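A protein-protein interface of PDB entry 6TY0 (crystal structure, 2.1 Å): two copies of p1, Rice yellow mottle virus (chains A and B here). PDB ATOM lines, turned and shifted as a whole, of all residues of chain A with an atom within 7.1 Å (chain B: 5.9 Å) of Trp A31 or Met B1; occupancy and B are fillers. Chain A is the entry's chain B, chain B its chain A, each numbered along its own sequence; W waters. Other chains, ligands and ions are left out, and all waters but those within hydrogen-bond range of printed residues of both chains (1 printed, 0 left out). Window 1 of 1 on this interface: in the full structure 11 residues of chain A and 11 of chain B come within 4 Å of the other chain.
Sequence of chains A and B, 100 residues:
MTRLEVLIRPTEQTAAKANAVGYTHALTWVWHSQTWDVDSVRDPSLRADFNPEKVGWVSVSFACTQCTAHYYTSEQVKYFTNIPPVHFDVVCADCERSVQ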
ATOM      1  N   MET A   1      15.309   8.600   4.712  1.00  0.00           N
ATOM      2  CA  MET A   1      14.358   9.570   4.108  1.00  0.00           C
ATOM      3  C   MET A   1      14.036   9.136   2.698  1.00  0.00           C
ATOM      4  O   MET A   1      14.623   8.191   2.205  1.00  0.00           O
ATOM      5  CB  MET A   1      14.863  11.035   4.190  1.00  0.00           C
ATOM      6  CG  MET A   1      16.338  11.350   4.013  1.00  0.00           C
ATOM      7  SD  MET A   1      16.771  12.927   4.829  1.00  0.00           S
ATOM      8  CE  MET A   1      15.274  13.916   4.711  1.00  0.00           C
ATOM      9  N   THR A   2      13.051   9.784   2.105  1.00  0.00           N
ATOM     10  CA  THR A   2      12.497   9.405   0.834  1.00  0.00           C
ATOM     11  C   THR A   2      12.905  10.454  -0.178  1.00  0.00           C
ATOM     12  O   THR A   2      13.116  11.622   0.186  1.00  0.00           O
ATOM     13  CB  THR A   2      10.992   9.438   0.930  1.00  0.00           C
ATOM     14  OG1 THR A   2      10.602   8.681   2.070  1.00  0.00           O
ATOM     15  CG2 THR A   2      10.335   8.897  -0.352  1.00  0.00           C
ATOM     16  N   ARG A   3      13.004  10.063  -1.443  1.00  0.00           N
ATOM     17  CA  ARG A   3      13.408  11.012  -2.473  1.00  0.00           C
ATOM     18  C   ARG A   3      12.209  11.290  -3.320  1.00  0.00           C
ATOM     19  O   ARG A   3      11.349  10.448  -3.528  1.00  0.00           O
ATOM     20  CB  ARG A   3      14.609  10.526  -3.311  1.00  0.00           C
ATOM     21  CG  ARG A   3      14.296  10.269  -4.791  1.00  0.00           C
ATOM     22  CD  ARG A   3      14.801   8.934  -5.160  1.00  0.00           C
ATOM     23  NE  ARG A   3      14.200   8.248  -6.289  1.00  0.00           N
ATOM     24  CZ  ARG A   3      12.971   7.788  -6.335  1.00  0.00           C
ATOM     25  NH1 ARG A   3      12.098   8.077  -5.398  1.00  0.00           N
ATOM     26  NH2 ARG A   3      12.586   7.089  -7.391  1.00  0.00           N
ATOM     27  N   LEU A   4      12.157  12.516  -3.817  1.00  0.00           N
ATOM     28  CA  LEU A   4      11.173  12.928  -4.767  1.00  0.00           C
ATOM     29  C   LEU A   4      11.955  13.247  -6.036  1.00  0.00           C
ATOM     30  O   LEU A   4      13.022  13.827  -5.978  1.00  0.00           O
ATOM     31  CB  LEU A   4      10.487  14.156  -4.207  1.00  0.00           C
ATOM     32  CG  LEU A   4       9.311  14.727  -4.945  1.00  0.00           C
ATOM     33  CD1 LEU A   4       8.094  13.828  -4.777  1.00  0.00           C
ATOM     34  CD2 LEU A   4       9.071  16.119  -4.396  1.00  0.00           C
ATOM     35  N   THR A  28      16.332  16.066 -10.873  1.00  0.00           N
ATOM     36  CA  THR A  28      16.849  16.441  -9.592  1.00  0.00           C
ATOM     37  C   THR A  28      16.172  15.588  -8.540  1.00  0.00           C
ATOM     38  O   THR A  28      14.965  15.333  -8.573  1.00  0.00           O
ATOM     39  CB  THR A  28      16.568  17.965  -9.328  1.00  0.00           C
ATOM     40  OG1 THR A  28      17.080  18.750 -10.416  1.00  0.00           O
ATOM     41  CG2 THR A  28      17.241  18.413  -8.103  1.00  0.00           C
ATOM     42  N   TRP A  29      16.965  15.137  -7.605  1.00  0.00           N
ATOM     43  CA  TRP A  29      16.437  14.447  -6.452  1.00  0.00           C
ATOM     44  C   TRP A  29      16.259  15.415  -5.304  1.00  0.00           C
ATOM     45  O   TRP A  29      17.143  16.224  -5.005  1.00  0.00           O
ATOM     46  CB  TRP A  29      17.397  13.335  -6.083  1.00  0.00           C
ATOM     47  CG  TRP A  29      17.110  12.104  -6.838  1.00  0.00           C
ATOM     48  CD1 TRP A  29      16.312  11.962  -7.964  1.00  0.00           C
ATOM     49  CD2 TRP A  29      17.575  10.800  -6.510  1.00  0.00           C
ATOM     50  NE1 TRP A  29      16.278  10.626  -8.347  1.00  0.00           N
ATOM     51  CE2 TRP A  29      17.045   9.903  -7.469  1.00  0.00           C
ATOM     52  CE3 TRP A  29      18.392  10.301  -5.498  1.00  0.00           C
ATOM     53  CZ2 TRP A  29      17.289   8.533  -7.414  1.00  0.00           C
ATOM     54  CZ3 TRP A  29      18.641   8.925  -5.458  1.00  0.00           C
ATOM     55  CH2 TRP A  29      18.093   8.076  -6.401  1.00  0.00           C
ATOM     56  N   VAL A  30      15.128  15.309  -4.637  1.00  0.00           N
ATOM     57  CA  VAL A  30      14.914  16.105  -3.444  1.00  0.00           C
ATOM     58  C   VAL A  30      14.554  15.135  -2.322  1.00  0.00           C
ATOM     59  O   VAL A  30      13.733  14.277  -2.500  1.00  0.00           O
ATOM     60  CB  VAL A  30      13.837  17.189  -3.789  1.00  0.00           C
ATOM     61  CG1 VAL A  30      12.935  17.549  -2.604  1.00  0.00           C
ATOM     62  CG2 VAL A  30      14.569  18.416  -4.329  1.00  0.00           C
ATOM     63  N   TRP A  31      15.196  15.273  -1.182  1.00  0.00           N
ATOM     64  CA  TRP A  31      14.978  14.398  -0.052  1.00  0.00           C
ATOM     65  C   TRP A  31      14.009  14.986   0.959  1.00  0.00           C
ATOM     66  O   TRP A  31      14.030  16.172   1.220  1.00  0.00           O
ATOM     67  CB  TRP A  31      16.316  14.173   0.607  1.00  0.00           C
ATOM     68  CG  TRP A  31      17.246  13.432  -0.287  1.00  0.00           C
ATOM     69  CD1 TRP A  31      18.249  13.946  -1.006  1.00  0.00           C
ATOM     70  CD2 TRP A  31      17.232  12.025  -0.557  1.00  0.00           C
ATOM     71  NE1 TRP A  31      18.916  12.939  -1.683  1.00  0.00           N
ATOM     72  CE2 TRP A  31      18.294  11.756  -1.435  1.00  0.00           C
ATOM     73  CE3 TRP A  31      16.442  10.965  -0.118  1.00  0.00           C
ATOM     74  CZ2 TRP A  31      18.589  10.471  -1.894  1.00  0.00           C
ATOM     75  CZ3 TRP A  31      16.727   9.671  -0.595  1.00  0.00           C
ATOM     76  CH2 TRP A  31      17.793   9.450  -1.473  1.00  0.00           C
ATOM     77  N   HIS A  32      13.163  14.149   1.519  1.00  0.00           N
ATOM     78  CA  HIS A  32      12.305  14.531   2.629  1.00  0.00           C
ATOM     79  C   HIS A  32      12.067  13.321   3.552  1.00  0.00           C
ATOM     80  O   HIS A  32      12.380  12.177   3.197  1.00  0.00           O
ATOM     81  CB  HIS A  32      10.973  15.060   2.132  1.00  0.00           C
ATOM     82  CG  HIS A  32      10.191  14.082   1.332  1.00  0.00           C
ATOM     83  ND1 HIS A  32       9.367  13.140   1.907  1.00  0.00           N
ATOM     84  CD2 HIS A  32      10.090  13.904  -0.003  1.00  0.00           C
ATOM     85  CE1 HIS A  32       8.807  12.408   0.961  1.00  0.00           C
ATOM     86  NE2 HIS A  32       9.242  12.840  -0.207  1.00  0.00           N
ATOM     87  N   SER A  33      11.464  13.570   4.709  1.00  0.00           N
ATOM     88  CA  SER A  33      11.244  12.524   5.684  1.00  0.00           C
ATOM     89  C   SER A  33       9.875  11.884   5.508  1.00  0.00           C
ATOM     90  O   SER A  33       9.057  12.267   4.639  1.00  0.00           O
ATOM     91  CB  SER A  33      11.389  13.098   7.095  1.00  0.00           C
ATOM     92  OG  SER A  33      10.190  13.773   7.453  1.00  0.00           O
ATOM     93  N   PHE A  62       7.059  21.881   1.766  1.00  0.00           N
ATOM     94  CA  PHE A  62       6.004  21.034   2.288  1.00  0.00           C
ATOM     95  C   PHE A  62       5.379  21.752   3.482  1.00  0.00           C
ATOM     96  O   PHE A  62       6.100  22.270   4.312  1.00  0.00           O
ATOM     97  CB  PHE A  62       6.599  19.732   2.786  1.00  0.00           C
ATOM     98  CG  PHE A  62       7.287  18.915   1.732  1.00  0.00           C
ATOM     99  CD1 PHE A  62       8.584  19.207   1.349  1.00  0.00           C
ATOM    100  CD2 PHE A  62       6.663  17.826   1.179  1.00  0.00           C
ATOM    101  CE1 PHE A  62       9.245  18.447   0.409  1.00  0.00           C
ATOM    102  CE2 PHE A  62       7.306  17.067   0.218  1.00  0.00           C
ATOM    103  CZ  PHE A  62       8.609  17.362  -0.143  1.00  0.00           C
ATOM    104  N   TYR A  71       8.420  21.818   5.891  1.00  0.00           N
ATOM    105  CA  TYR A  71       9.771  21.529   5.506  1.00  0.00           C
ATOM    106  C   TYR A  71      10.038  22.272   4.212  1.00  0.00           C
ATOM    107  O   TYR A  71       9.141  22.455   3.414  1.00  0.00           O
ATOM    108  CB  TYR A  71       9.921  20.007   5.274  1.00  0.00           C
ATOM    109  CG  TYR A  71      11.286  19.521   4.882  1.00  0.00           C
ATOM    110  CD1 TYR A  71      12.334  19.602   5.735  1.00  0.00           C
ATOM    111  CD2 TYR A  71      11.509  18.914   3.648  1.00  0.00           C
ATOM    112  CE1 TYR A  71      13.596  19.153   5.382  1.00  0.00           C
ATOM    113  CE2 TYR A  71      12.767  18.498   3.273  1.00  0.00           C
ATOM    114  CZ  TYR A  71      13.812  18.611   4.150  1.00  0.00           C
ATOM    115  OH  TYR A  71      15.091  18.146   3.823  1.00  0.00           O
ATOM    116  N   TYR A  72      11.290  22.651   4.012  1.00  0.00           N
ATOM    117  CA  TYR A  72      11.675  23.408   2.883  1.00  0.00           C
ATOM    118  C   TYR A  72      13.008  22.872   2.453  1.00  0.00           C
ATOM    119  O   TYR A  72      13.894  22.620   3.282  1.00  0.00           O
ATOM    120  CB  TYR A  72      11.762  24.912   3.251  1.00  0.00           C
ATOM    121  CG  TYR A  72      12.269  25.762   2.117  1.00  0.00           C
ATOM    122  CD1 TYR A  72      13.633  25.899   1.928  1.00  0.00           C
ATOM    123  CD2 TYR A  72      11.398  26.387   1.219  1.00  0.00           C
ATOM    124  CE1 TYR A  72      14.142  26.639   0.914  1.00  0.00           C
ATOM    125  CE2 TYR A  72      11.907  27.136   0.170  1.00  0.00           C
ATOM    126  CZ  TYR A  72      13.282  27.257   0.044  1.00  0.00           C
ATOM    127  OH  TYR A  72      13.896  27.975  -0.914  1.00  0.00           O
ATOM    128  N   THR A  73      13.133  22.652   1.150  1.00  0.00           N
ATOM    129  CA  THR A  73      14.400  22.279   0.585  1.00  0.00           C
ATOM    130  C   THR A  73      14.602  22.849  -0.831  1.00  0.00           C
ATOM    131  O   THR A  73      13.658  23.146  -1.536  1.00  0.00           O
ATOM    132  CB  THR A  73      14.592  20.754   0.656  1.00  0.00           C
ATOM    133  OG1 THR A  73      15.945  20.453   0.349  1.00  0.00           O
ATOM    134  CG2 THR A  73      13.641  20.013  -0.233  1.00  0.00           C
ATOM    135  N   SER A  74      15.841  23.074  -1.199  1.00  0.00           N
ATOM    136  CA  SER A  74      16.158  23.673  -2.478  1.00  0.00           C
ATOM    137  C   SER A  74      17.505  23.122  -2.951  1.00  0.00           C
ATOM    138  O   SER A  74      18.354  22.790  -2.134  1.00  0.00           O
ATOM    139  CB  SER A  74      16.199  25.206  -2.403  1.00  0.00           C
ATOM    140  OG  SER A  74      17.359  25.572  -1.708  1.00  0.00           O
ATOM    141  N   GLU A  75      17.646  22.959  -4.270  1.00  0.00           N
ATOM    142  CA  GLU A  75      18.839  22.414  -4.890  1.00  0.00           C
ATOM    143  C   GLU A  75      19.174  23.195  -6.187  1.00  0.00           C
ATOM    144  O   GLU A  75      18.272  23.652  -6.893  1.00  0.00           O
ATOM    145  CB  GLU A  75      18.545  20.925  -5.188  1.00  0.00           C
ATOM    146  CG  GLU A  75      19.606  20.152  -5.981  1.00  0.00           C
ATOM    147  CD  GLU A  75      20.981  20.195  -5.329  1.00  0.00           C
ATOM    148  OE1 GLU A  75      21.087  20.594  -4.145  1.00  0.00           O
ATOM    149  OE2 GLU A  75      21.975  19.833  -6.001  1.00  0.00           O
ATOM    150  N   GLN A  76      20.449  23.337  -6.506  1.00  0.00           N
ATOM    151  CA  GLN A  76      20.861  23.920  -7.788  1.00  0.00           C
ATOM    152  C   GLN A  76      20.580  23.040  -9.007  1.00  0.00           C
ATOM    153  O   GLN A  76      20.694  21.803  -8.943  1.00  0.00           O
ATOM    154  CB  GLN A  76      22.361  24.233  -7.773  1.00  0.00           C
ATOM    155  CG  GLN A  76      22.628  25.546  -7.085  1.00  0.00           C
ATOM    156  CD  GLN A  76      24.070  25.971  -7.185  1.00  0.00           C
ATOM    157  OE1 GLN A  76      24.983  25.141  -7.208  1.00  0.00           O
ATOM    158  NE2 GLN A  76      24.284  27.282  -7.241  1.00  0.00           N
ATOM    159  N   MET B   1      23.847  18.868  -3.988  1.00  0.00           N
ATOM    160  CA  MET B   1      23.414  17.628  -3.262  1.00  0.00           C
ATOM    161  C   MET B   1      24.627  17.019  -2.602  1.00  0.00           C
ATOM    162  O   MET B   1      25.430  16.403  -3.295  1.00  0.00           O
ATOM    163  CB  MET B   1      22.817  16.616  -4.254  1.00  0.00           C
ATOM    164  CG  MET B   1      22.053  15.484  -3.594  1.00  0.00           C
ATOM    165  SD  MET B   1      20.852  16.231  -2.478  1.00  0.00           S
ATOM    166  CE  MET B   1      19.581  16.737  -3.641  1.00  0.00           C
ATOM    167  N   THR B   2      24.810  17.243  -1.304  1.00  0.00           N
ATOM    168  CA  THR B   2      25.965  16.709  -0.590  1.00  0.00           C
ATOM    169  C   THR B   2      25.448  15.895   0.602  1.00  0.00           C
ATOM    170  O   THR B   2      24.572  16.352   1.325  1.00  0.00           O
ATOM    171  CB  THR B   2      26.900  17.822  -0.062  1.00  0.00           C
ATOM    172  OG1 THR B   2      27.280  18.707  -1.123  1.00  0.00           O
ATOM    173  CG2 THR B   2      28.170  17.228   0.619  1.00  0.00           C
ATOM    174  N   ARG B   3      25.974  14.688   0.785  1.00  0.00           N
ATOM    175  CA  ARG B   3      25.596  13.836   1.907  1.00  0.00           C
ATOM    176  C   ARG B   3      26.385  14.267   3.150  1.00  0.00           C
ATOM    177  O   ARG B   3      27.595  14.477   3.084  1.00  0.00           O
ATOM    178  CB  ARG B   3      25.924  12.390   1.588  1.00  0.00           C
ATOM    179  CG  ARG B   3      25.418  11.376   2.587  1.00  0.00           C
ATOM    180  CD  ARG B   3      26.142  10.048   2.356  1.00  0.00           C
ATOM    181  NE  ARG B   3      25.883   9.463   1.028  1.00  0.00           N
ATOM    182  CZ  ARG B   3      25.097   8.404   0.776  1.00  0.00           C
ATOM    183  NH1 ARG B   3      24.430   7.780   1.756  1.00  0.00           N
ATOM    184  NH2 ARG B   3      24.977   7.952  -0.468  1.00  0.00           N
ATOM    185  N   TRP B  31      21.114  15.283   3.888  1.00  0.00           N
ATOM    186  CA  TRP B  31      21.590  15.970   2.695  1.00  0.00           C
ATOM    187  C   TRP B  31      21.458  17.482   2.809  1.00  0.00           C
ATOM    188  O   TRP B  31      20.541  18.013   3.462  1.00  0.00           O
ATOM    189  CB  TRP B  31      20.750  15.532   1.504  1.00  0.00           C
ATOM    190  CG  TRP B  31      20.716  14.028   1.345  1.00  0.00           C
ATOM    191  CD1 TRP B  31      19.831  13.142   1.933  1.00  0.00           C
ATOM    192  CD2 TRP B  31      21.604  13.233   0.548  1.00  0.00           C
ATOM    193  NE1 TRP B  31      20.120  11.858   1.555  1.00  0.00           N
ATOM    194  CE2 TRP B  31      21.200  11.872   0.708  1.00  0.00           C
ATOM    195  CE3 TRP B  31      22.707  13.535  -0.286  1.00  0.00           C
ATOM    196  CZ2 TRP B  31      21.854  10.820   0.078  1.00  0.00           C
ATOM    197  CZ3 TRP B  31      23.377  12.468  -0.933  1.00  0.00           C
ATOM    198  CH2 TRP B  31      22.940  11.119  -0.733  1.00  0.00           C
ATOM    199  N   HIS B  32      22.355  18.174   2.135  1.00  0.00           N
ATOM    200  CA  HIS B  32      22.265  19.602   2.034  1.00  0.00           C
ATOM    201  C   HIS B  32      22.745  20.093   0.666  1.00  0.00           C
ATOM    202  O   HIS B  32      23.406  19.378  -0.061  1.00  0.00           O
ATOM    203  CB  HIS B  32      23.080  20.235   3.160  1.00  0.00           C
ATOM    204  CG  HIS B  32      24.549  20.022   3.054  1.00  0.00           C
ATOM    205  ND1 HIS B  32      25.340  20.716   2.156  1.00  0.00           N
ATOM    206  CD2 HIS B  32      25.391  19.264   3.789  1.00  0.00           C
ATOM    207  CE1 HIS B  32      26.609  20.392   2.351  1.00  0.00           C
ATOM    208  NE2 HIS B  32      26.664  19.493   3.317  1.00  0.00           N
ATOM    209  N   SER B  33      22.407  21.328   0.366  1.00  0.00           N
ATOM    210  CA  SER B  33      22.687  21.965  -0.896  1.00  0.00           C
ATOM    211  C   SER B  33      24.040  22.598  -0.898  1.00  0.00           C
ATOM    212  O   SER B  33      24.796  22.561   0.088  1.00  0.00           O
ATOM    213  CB  SER B  33      21.604  23.028  -1.183  1.00  0.00           C
ATOM    214  OG  SER B  33      21.786  24.151  -0.334  1.00  0.00           O
ATOM    215  N   GLN B  34      24.332  23.222  -2.033  1.00  0.00           N
ATOM    216  CA  GLN B  34      25.611  23.880  -2.278  1.00  0.00           C
ATOM    217  C   GLN B  34      25.873  25.035  -1.323  1.00  0.00           C
ATOM    218  O   GLN B  34      27.020  25.331  -1.016  1.00  0.00           O
ATOM    219  CB  GLN B  34      25.636  24.392  -3.732  1.00  0.00           C
ATOM    220  CG  GLN B  34      25.601  23.278  -4.788  1.00  0.00           C
ATOM    221  CD  GLN B  34      24.246  22.581  -5.051  1.00  0.00           C
ATOM    222  OE1 GLN B  34      23.164  22.955  -4.551  1.00  0.00           O
ATOM    223  NE2 GLN B  34      24.320  21.525  -5.872  1.00  0.00           N
ATOM    224  N   ASP B  37      28.224  23.797   1.391  1.00  0.00           N
ATOM    225  CA  ASP B  37      29.535  23.229   1.036  1.00  0.00           C
ATOM    226  C   ASP B  37      30.671  24.179   1.413  1.00  0.00           C
ATOM    227  O   ASP B  37      31.223  24.878   0.558  1.00  0.00           O
ATOM    228  CB  ASP B  37      29.606  22.969  -0.471  1.00  0.00           C
ATOM    229  CG  ASP B  37      28.722  21.810  -0.906  1.00  0.00           C
ATOM    230  OD1 ASP B  37      28.554  20.848  -0.121  1.00  0.00           O
ATOM    231  OD2 ASP B  37      28.187  21.866  -2.037  1.00  0.00           O
ATOM    232  N   TYR B  71      18.717  26.331   7.032  1.00  0.00           N
ATOM    233  CA  TYR B  71      18.181  25.054   6.539  1.00  0.00           C
ATOM    234  C   TYR B  71      18.097  24.105   7.737  1.00  0.00           C
ATOM    235  O   TYR B  71      18.947  24.120   8.609  1.00  0.00           O
ATOM    236  CB  TYR B  71      19.095  24.496   5.420  1.00  0.00           C
ATOM    237  CG  TYR B  71      18.739  23.117   4.949  1.00  0.00           C
ATOM    238  CD1 TYR B  71      17.536  22.876   4.342  1.00  0.00           C
ATOM    239  CD2 TYR B  71      19.625  22.056   5.106  1.00  0.00           C
ATOM    240  CE1 TYR B  71      17.186  21.610   3.930  1.00  0.00           C
ATOM    241  CE2 TYR B  71      19.298  20.779   4.673  1.00  0.00           C
ATOM    242  CZ  TYR B  71      18.098  20.580   4.068  1.00  0.00           C
ATOM    243  OH  TYR B  71      17.753  19.352   3.694  1.00  0.00           O
ATOM    244  N   THR B  73      17.015  19.990   8.617  1.00  0.00           N
ATOM    245  CA  THR B  73      16.569  18.629   8.302  1.00  0.00           C
ATOM    246  C   THR B  73      16.654  17.759   9.523  1.00  0.00           C
ATOM    247  O   THR B  73      17.338  18.060  10.529  1.00  0.00           O
ATOM    248  CB  THR B  73      17.474  17.803   7.379  1.00  0.00           C
ATOM    249  OG1 THR B  73      18.791  18.361   7.259  1.00  0.00           O
ATOM    250  CG2 THR B  73      16.818  17.548   6.162  1.00  0.00           C
HETATM  251  O   HOH W   1      18.399  15.868   4.250  1.00  0.00           O
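Trp A31 touches Met B1, but with the chains exchanged Met A1 does not touch Trp B31 (4.2 Å). Trp B31 touches its own counterpart, Trp A31. Tyr A71 touches its own counterpart, Tyr B71. Tyr A71 touches Thr B73, and with the chains exchanged Thr A73 touches Tyr B71. Positions printed for both chains: 1, 2, 3, 31, 32, 33, 71 and 73. Of the 12 pairs that touch across the chains among the printed residues, 4 have their exchanged pair printed and touching as well.
Among the printed residues, merely in contact across the chains: Trp A29 with Met B1, Trp A31 with Met B1, Trp A31 with Trp B31, Tyr A71 with Thr B73, Tyr A72 with Tyr B71, Thr A73 with Tyr B71, Ser A74 with Ser B33 and Glu A75 with Ser B33.
Ser A33 touches none of the printed residues of chain B. Printed residues of chain B within 4 Å of Tyr A72: Tyr B71 (3.5 Å). Met B1 touches three residues of chain A. Of the printed residues of chain A, Gln B34 touches Glu A75 (2.9 Å) and Gln A76 (3.1 Å). Of the printed residues of chain A, Tyr B71 touches Tyr A71, Tyr A72 and Thr A73. The nearest residue of chain B that does not touch Trp A31 is Tyr B71 (5.5 Å).
NE2 of Gln B34 sits close to N of Met B1 (3.3 Å). OH of Tyr B71 is in hydrogen-bond range of O of Trp B31 (3.1 Å). The side-chain hydroxyl (OH) of Tyr A71 lies close to the backbone carbonyl oxygen (O) of Trp A31 (3.4 Å). The backbone NH (N) of Phe A62 sits at hydrogen-bond distance from the backbone carbonyl oxygen (O) of Tyr A71, at 2.7 Å.
The side-chain carboxylate (OE2) of Glu A75 sits at hydrogen-bond distance from the backbone NH (N) of Met B1, 2.9 Å away. The side-chain amide nitrogen (NE2) of Gln B34 sits at hydrogen-bond distance from the side-chain carboxylate (OE2) of Glu A75. The side-chain amide oxygen (OE1) of Gln B34 is in hydrogen-bond range of the backbone NH (N) of Gln A76 (3.4 Å). The side-chain hydroxyl (OH) of Tyr B71 sits at hydrogen-bond distance from the side-chain hydroxyl (OH) of Tyr A71, at 2.9 Å.
Water W1 lies within hydrogen-bond range of N of Trp B31 (2.8 Å) and SD of Met A1 (3.4 Å).
Hydrophobic or aromatic side chains of chain B within 4 Å of the printed part of chain A: Met B1, Trp B31 and Tyr B71. Of the 17 printed residues of chain A, 8 touch a printed residue of chain B. Hydrophobic or aromatic side chains of chain A that line the printed part of chain B: Trp A31 and Tyr A71. Among the printed residues, 12 pairs touch across the chains. Among the printed residues, no Asp or Glu carboxylate lies within 4 Å of a Lys or Arg side-chain nitrogen of the other chain.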
